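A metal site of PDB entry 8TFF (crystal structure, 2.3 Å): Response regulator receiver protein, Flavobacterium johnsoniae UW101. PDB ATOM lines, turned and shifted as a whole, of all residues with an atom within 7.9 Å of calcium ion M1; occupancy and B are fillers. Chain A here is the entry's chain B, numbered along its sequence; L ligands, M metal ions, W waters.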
ATOM      1  N   VAL A 238      21.392   5.886  21.907  1.00  0.00           N
ATOM      2  CA  VAL A 238      20.711   7.030  22.464  1.00  0.00           C
ATOM      3  C   VAL A 238      21.374   8.287  21.918  1.00  0.00           C
ATOM      4  O   VAL A 238      22.468   8.649  22.344  1.00  0.00           O
ATOM      5  CB  VAL A 238      20.707   6.981  24.012  1.00  0.00           C
ATOM      6  CG1 VAL A 238      19.977   8.166  24.632  1.00  0.00           C
ATOM      7  CG2 VAL A 238      20.113   5.662  24.519  1.00  0.00           C
ATOM      8  N   ILE A 239      20.699   8.903  20.933  1.00  0.00           N
ATOM      9  CA  ILE A 239      21.079  10.220  20.451  1.00  0.00           C
ATOM     10  C   ILE A 239      20.522  11.234  21.439  1.00  0.00           C
ATOM     11  O   ILE A 239      19.314  11.380  21.541  1.00  0.00           O
ATOM     12  CB  ILE A 239      20.584  10.502  19.027  1.00  0.00           C
ATOM     13  CG1 ILE A 239      20.911   9.375  18.047  1.00  0.00           C
ATOM     14  CG2 ILE A 239      21.156  11.847  18.578  1.00  0.00           C
ATOM     15  CD1 ILE A 239      20.409   9.579  16.648  1.00  0.00           C
ATOM     16  N   ASP A 240      21.395  11.936  22.165  1.00  0.00           N
ATOM     17  CA  ASP A 240      20.952  12.934  23.111  1.00  0.00           C
ATOM     18  C   ASP A 240      20.222  14.040  22.329  1.00  0.00           C
ATOM     19  O   ASP A 240      20.702  14.496  21.286  1.00  0.00           O
ATOM     20  CB  ASP A 240      22.103  13.529  23.931  1.00  0.00           C
ATOM     21  CG  ASP A 240      21.600  14.302  25.148  1.00  0.00           C
ATOM     22  OD1 ASP A 240      21.677  13.767  26.280  1.00  0.00           O
ATOM     23  OD2 ASP A 240      21.043  15.393  24.979  1.00  0.00           O
ATOM     24  N   ASN A 241      19.040  14.411  22.841  1.00  0.00           N
ATOM     25  CA  ASN A 241      18.370  15.653  22.482  1.00  0.00           C
ATOM     26  C   ASN A 241      17.796  15.575  21.060  1.00  0.00           C
ATOM     27  O   ASN A 241      17.862  16.542  20.336  1.00  0.00           O
ATOM     28  CB  ASN A 241      19.282  16.885  22.575  1.00  0.00           C
ATOM     29  CG  ASN A 241      18.546  18.165  22.903  1.00  0.00           C
ATOM     30  OD1 ASN A 241      17.306  18.204  22.910  1.00  0.00           O
ATOM     31  ND2 ASN A 241      19.294  19.225  23.149  1.00  0.00           N
ATOM     32  N   LEU A 242      17.240  14.429  20.672  1.00  0.00           N
ATOM     33  CA  LEU A 242      16.634  14.285  19.360  1.00  0.00           C
ATOM     34  C   LEU A 242      15.135  14.586  19.427  1.00  0.00           C
ATOM     35  O   LEU A 242      14.382  13.842  20.049  1.00  0.00           O
ATOM     36  CB  LEU A 242      16.851  12.863  18.825  1.00  0.00           C
ATOM     37  CG  LEU A 242      16.612  12.664  17.325  1.00  0.00           C
ATOM     38  CD1 LEU A 242      17.763  13.211  16.509  1.00  0.00           C
ATOM     39  CD2 LEU A 242      16.418  11.202  16.992  1.00  0.00           C
ATOM     40  N   THR A 272      12.845  17.428  31.509  1.00  0.00           N
ATOM     41  CA  THR A 272      13.207  16.875  30.215  1.00  0.00           C
ATOM     42  C   THR A 272      14.659  17.256  29.908  1.00  0.00           C
ATOM     43  O   THR A 272      14.928  18.117  29.077  1.00  0.00           O
ATOM     44  CB  THR A 272      12.249  17.338  29.109  1.00  0.00           C
ATOM     45  OG1 THR A 272      12.016  18.742  29.221  1.00  0.00           O
ATOM     46  CG2 THR A 272      10.911  16.643  29.153  1.00  0.00           C
ATOM     47  N   ALA A 273      15.580  16.625  30.646  1.00  0.00           N
ATOM     48  CA  ALA A 273      16.986  17.004  30.700  1.00  0.00           C
ATOM     49  C   ALA A 273      17.836  15.778  31.028  1.00  0.00           C
ATOM     50  O   ALA A 273      17.399  14.872  31.751  1.00  0.00           O
ATOM     51  CB  ALA A 273      17.212  18.130  31.686  1.00  0.00           C
ATOM     52  N   THR A 274      19.056  15.780  30.493  1.00  0.00           N
ATOM     53  CA  THR A 274      19.945  14.624  30.452  1.00  0.00           C
ATOM     54  C   THR A 274      20.209  14.014  31.836  1.00  0.00           C
ATOM     55  O   THR A 274      20.115  12.794  32.009  1.00  0.00           O
ATOM     56  CB  THR A 274      21.282  15.049  29.827  1.00  0.00           C
ATOM     57  OG1 THR A 274      20.976  15.922  28.720  1.00  0.00           O
ATOM     58  CG2 THR A 274      22.115  13.856  29.418  1.00  0.00           C
ATOM     59  N   GLN A 275      20.557  14.870  32.802  1.00  0.00           N
ATOM     60  CA  GLN A 275      20.839  14.478  34.168  1.00  0.00           C
ATOM     61  C   GLN A 275      19.724  13.610  34.756  1.00  0.00           C
ATOM     62  O   GLN A 275      19.995  12.706  35.524  1.00  0.00           O
ATOM     63  CB  GLN A 275      21.036  15.739  34.985  1.00  0.00           C
ATOM     64  CG  GLN A 275      21.162  15.515  36.486  1.00  0.00           C
ATOM     65  CD  GLN A 275      21.255  16.838  37.201  1.00  0.00           C
ATOM     66  OE1 GLN A 275      21.181  17.904  36.574  1.00  0.00           O
ATOM     67  NE2 GLN A 275      21.392  16.801  38.507  1.00  0.00           N
ATOM     68  N   TYR A 276      18.478  13.889  34.413  1.00  0.00           N
ATOM     69  CA  TYR A 276      17.341  13.204  35.007  1.00  0.00           C
ATOM     70  C   TYR A 276      16.892  12.081  34.081  1.00  0.00           C
ATOM     71  O   TYR A 276      16.941  10.913  34.456  1.00  0.00           O
ATOM     72  CB  TYR A 276      16.268  14.254  35.304  1.00  0.00           C
ATOM     73  CG  TYR A 276      16.663  15.234  36.364  1.00  0.00           C
ATOM     74  CD1 TYR A 276      16.432  14.964  37.704  1.00  0.00           C
ATOM     75  CD2 TYR A 276      17.348  16.392  36.053  1.00  0.00           C
ATOM     76  CE1 TYR A 276      16.794  15.852  38.699  1.00  0.00           C
ATOM     77  CE2 TYR A 276      17.755  17.286  37.034  1.00  0.00           C
ATOM     78  CZ  TYR A 276      17.474  17.015  38.367  1.00  0.00           C
ATOM     79  OH  TYR A 276      17.844  17.893  39.336  1.00  0.00           O
ATOM     80  N   ALA A 277      16.463  12.440  32.865  1.00  0.00           N
ATOM     81  CA  ALA A 277      15.777  11.496  32.003  1.00  0.00           C
ATOM     82  C   ALA A 277      16.760  10.477  31.439  1.00  0.00           C
ATOM     83  O   ALA A 277      16.378   9.319  31.232  1.00  0.00           O
ATOM     84  CB  ALA A 277      15.076  12.214  30.864  1.00  0.00           C
ATOM     85  N   ARG A 278      18.008  10.888  31.141  1.00  0.00           N
ATOM     86  CA  ARG A 278      18.895   9.936  30.480  1.00  0.00           C
ATOM     87  C   ARG A 278      19.384   8.889  31.488  1.00  0.00           C
ATOM     88  O   ARG A 278      19.432   7.705  31.169  1.00  0.00           O
ATOM     89  CB  ARG A 278      20.053  10.599  29.716  1.00  0.00           C
ATOM     90  CG  ARG A 278      20.526   9.746  28.544  1.00  0.00           C
ATOM     91  CD  ARG A 278      21.528  10.384  27.592  1.00  0.00           C
ATOM     92  NE  ARG A 278      22.853  10.446  28.174  1.00  0.00           N
ATOM     93  CZ  ARG A 278      23.839  11.266  27.833  1.00  0.00           C
ATOM     94  NH1 ARG A 278      23.670  12.215  26.928  1.00  0.00           N
ATOM     95  NH2 ARG A 278      25.029  11.141  28.402  1.00  0.00           N
ATOM     96  N   ASN A 308      26.296  12.957  34.098  1.00  0.00           N
ATOM     97  CA  ASN A 308      26.008  11.663  33.482  1.00  0.00           C
ATOM     98  C   ASN A 308      27.300  10.864  33.342  1.00  0.00           C
ATOM     99  O   ASN A 308      27.552  10.250  32.302  1.00  0.00           O
ATOM    100  CB  ASN A 308      25.290  11.863  32.142  1.00  0.00           C
ATOM    101  CG  ASN A 308      23.856  12.321  32.300  1.00  0.00           C
ATOM    102  OD1 ASN A 308      22.907  11.524  32.212  1.00  0.00           O
ATOM    103  ND2 ASN A 308      23.657  13.614  32.538  1.00  0.00           N
ATOM    104  N   GLU A 311      26.595   6.195  33.755  1.00  0.00           N
ATOM    105  CA  GLU A 311      25.480   5.581  33.054  1.00  0.00           C
ATOM    106  C   GLU A 311      25.769   4.099  32.814  1.00  0.00           C
ATOM    107  O   GLU A 311      24.847   3.284  32.889  1.00  0.00           O
ATOM    108  CB  GLU A 311      25.174   6.339  31.746  1.00  0.00           C
ATOM    109  CG  GLU A 311      24.637   7.747  31.969  1.00  0.00           C
ATOM    110  CD  GLU A 311      24.184   8.469  30.709  1.00  0.00           C
ATOM    111  OE1 GLU A 311      24.922   8.338  29.668  1.00  0.00           O
ATOM    112  OE2 GLU A 311      23.118   9.192  30.761  1.00  0.00           O
ATOM    113  N   VAL A 358      25.763   6.181  23.462  1.00  0.00           N
ATOM    114  CA  VAL A 358      25.253   7.529  23.643  1.00  0.00           C
ATOM    115  C   VAL A 358      26.061   8.433  22.726  1.00  0.00           C
ATOM    116  O   VAL A 358      27.286   8.386  22.736  1.00  0.00           O
ATOM    117  CB  VAL A 358      25.407   7.982  25.114  1.00  0.00           C
ATOM    118  CG1 VAL A 358      25.055   9.453  25.308  1.00  0.00           C
ATOM    119  CG2 VAL A 358      24.586   7.125  26.067  1.00  0.00           C
ATOM    120  N   ASN A 360      26.335  12.423  21.618  1.00  0.00           N
ATOM    121  CA  ASN A 360      25.996  13.744  22.143  1.00  0.00           C
ATOM    122  C   ASN A 360      25.941  14.858  21.087  1.00  0.00           C
ATOM    123  O   ASN A 360      25.599  15.995  21.387  1.00  0.00           O
ATOM    124  CB  ASN A 360      26.968  14.161  23.260  1.00  0.00           C
ATOM    125  CG  ASN A 360      26.617  13.559  24.613  1.00  0.00           C
ATOM    126  OD1 ASN A 360      25.565  12.966  24.797  1.00  0.00           O
ATOM    127  ND2 ASN A 360      27.478  13.754  25.588  1.00  0.00           N
ATOM    128  N   ASP A 363      22.760  17.252  20.682  1.00  0.00           N
ATOM    129  CA  ASP A 363      22.778  18.115  21.860  1.00  0.00           C
ATOM    130  C   ASP A 363      23.755  19.269  21.676  1.00  0.00           C
ATOM    131  O   ASP A 363      23.411  20.389  21.978  1.00  0.00           O
ATOM    132  CB  ASP A 363      23.150  17.361  23.141  1.00  0.00           C
ATOM    133  CG  ASP A 363      22.938  18.226  24.367  1.00  0.00           C
ATOM    134  OD1 ASP A 363      21.774  18.579  24.631  1.00  0.00           O
ATOM    135  OD2 ASP A 363      23.942  18.640  24.972  1.00  0.00           O
ATOM    136  N   HIS A 367      22.869  23.701  21.304  1.00  0.00           N
ATOM    137  CA  HIS A 367      23.400  24.798  22.109  1.00  0.00           C
ATOM    138  C   HIS A 367      24.277  25.701  21.244  1.00  0.00           C
ATOM    139  O   HIS A 367      24.315  26.913  21.460  1.00  0.00           O
ATOM    140  CB  HIS A 367      24.120  24.284  23.360  1.00  0.00           C
ATOM    141  CG  HIS A 367      23.188  23.641  24.316  1.00  0.00           C
ATOM    142  ND1 HIS A 367      22.012  24.258  24.688  1.00  0.00           N
ATOM    143  CD2 HIS A 367      23.203  22.450  24.926  1.00  0.00           C
ATOM    144  CE1 HIS A 367      21.345  23.466  25.508  1.00  0.00           C
ATOM    145  NE2 HIS A 367      22.050  22.361  25.672  1.00  0.00           N
ATOM    146  N   THR A 416      16.146   8.411  22.245  1.00  0.00           N
ATOM    147  CA  THR A 416      16.687   9.634  22.789  1.00  0.00           C
ATOM    148  C   THR A 416      16.175   9.814  24.220  1.00  0.00           C
ATOM    149  O   THR A 416      15.323   9.048  24.671  1.00  0.00           O
ATOM    150  CB  THR A 416      16.288  10.828  21.915  1.00  0.00           C
ATOM    151  OG1 THR A 416      16.879  12.031  22.418  1.00  0.00           O
ATOM    152  CG2 THR A 416      14.796  11.030  21.826  1.00  0.00           C
ATOM    153  N   ASP A 417      16.685  10.835  24.914  1.00  0.00           N
ATOM    154  CA  ASP A 417      16.298  11.113  26.272  1.00  0.00           C
ATOM    155  C   ASP A 417      15.231  12.206  26.354  1.00  0.00           C
ATOM    156  O   ASP A 417      14.466  12.214  27.313  1.00  0.00           O
ATOM    157  CB  ASP A 417      17.507  11.497  27.132  1.00  0.00           C
ATOM    158  CG  ASP A 417      18.337  12.655  26.617  1.00  0.00           C
ATOM    159  OD1 ASP A 417      18.230  12.953  25.421  1.00  0.00           O
ATOM    160  OD2 ASP A 417      19.090  13.243  27.430  1.00  0.00           O
ATOM    161  N   HIS A 418      15.185  13.131  25.379  1.00  0.00           N
ATOM    162  CA  HIS A 418      14.262  14.260  25.368  1.00  0.00           C
ATOM    163  C   HIS A 418      14.570  15.094  24.125  1.00  0.00           C
ATOM    164  O   HIS A 418      15.616  14.914  23.510  1.00  0.00           O
ATOM    165  CB  HIS A 418      14.376  15.136  26.630  1.00  0.00           C
ATOM    166  CG  HIS A 418      15.732  15.724  26.735  1.00  0.00           C
ATOM    167  ND1 HIS A 418      16.189  16.762  25.960  1.00  0.00           N
ATOM    168  CD2 HIS A 418      16.758  15.369  27.519  1.00  0.00           C
ATOM    169  CE1 HIS A 418      17.452  17.020  26.265  1.00  0.00           C
ATOM    170  NE2 HIS A 418      17.827  16.193  27.222  1.00  0.00           N
ATOM    171  N   GLY A 419      13.614  15.936  23.727  1.00  0.00           N
ATOM    172  CA  GLY A 419      13.809  16.880  22.648  1.00  0.00           C
ATOM    173  C   GLY A 419      14.036  18.277  23.200  1.00  0.00           C
ATOM    174  O   GLY A 419      14.463  18.465  24.347  1.00  0.00           O
ATOM    175  N   HIS A 502      15.563  22.942  26.778  1.00  0.00           N
ATOM    176  CA  HIS A 502      14.842  21.750  27.182  1.00  0.00           C
ATOM    177  C   HIS A 502      14.799  21.724  28.693  1.00  0.00           C
ATOM    178  O   HIS A 502      15.503  22.484  29.344  1.00  0.00           O
ATOM    179  CB  HIS A 502      15.504  20.516  26.586  1.00  0.00           C
ATOM    180  CG  HIS A 502      16.922  20.373  26.973  1.00  0.00           C
ATOM    181  ND1 HIS A 502      17.297  19.783  28.161  1.00  0.00           N
ATOM    182  CD2 HIS A 502      18.040  20.736  26.363  1.00  0.00           C
ATOM    183  CE1 HIS A 502      18.611  19.843  28.261  1.00  0.00           C
ATOM    184  NE2 HIS A 502      19.088  20.406  27.173  1.00  0.00           N
HETATM  185 BE1  LIG L   1      22.462  18.647  28.992  1.00  0.00          BE
HETATM  186  F1  LIG L   1      23.370  20.150  28.900  1.00  0.00           F
HETATM  187  F2  LIG L   1      20.826  18.734  29.730  1.00  0.00           F
HETATM  188  F3  LIG L   1      23.234  17.176  28.346  1.00  0.00           F
HETATM  189 CA    CA M   1      19.921  15.147  26.966  1.00  0.00          CA
HETATM  190 CA    CA M   2      21.865  20.602  26.514  1.00  0.00          CA
HETATM  191  O   HOH W   1      20.570  17.639  26.702  1.00  0.00           O
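The backbone carbonyl oxygen (O) of His 418 is in hydrogen-bond range of the side-chain hydroxyl (OG1) of Thr 416. The side-chain carboxylate (OD1) of Asp 240 sits close to the guanidinium group (NH1) of Arg 278 (2.6 Å). OG1 of Thr 416 is in hydrogen-bond range of OD1 of Asp 417 (3.4 Å). O of Thr 274 sits close to OD1 of Asn 308 (3.1 Å). OD1 of Asp 417 is in hydrogen-bond range of N of Asn 241 (3.1 Å). The backbone carbonyl oxygen (O) of His 418 lies within hydrogen-bond range of the backbone NH (N) of Leu 242. The backbone carbonyl oxygen of Asp 240 sits at hydrogen-bond distance from the backbone NH of Asp 363 (3.5 Å).
Calcium ion M1 is bound by the side-chain carboxylate (OD2) of Asp 417 (2.1 Å), the side-chain hydroxyl (OG1) of Thr 274 (2.2 Å), the side-chain carboxylate (OD2) of Asp 240 (2.3 Å), the side-chain carboxylate (OD1) of Asp 240 (2.3 Å), a ring nitrogen (NE2) of His 418 (2.4 Å) and water W1 (2.6 Å). Calcium ion M1 has six donor atoms within binding distance.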
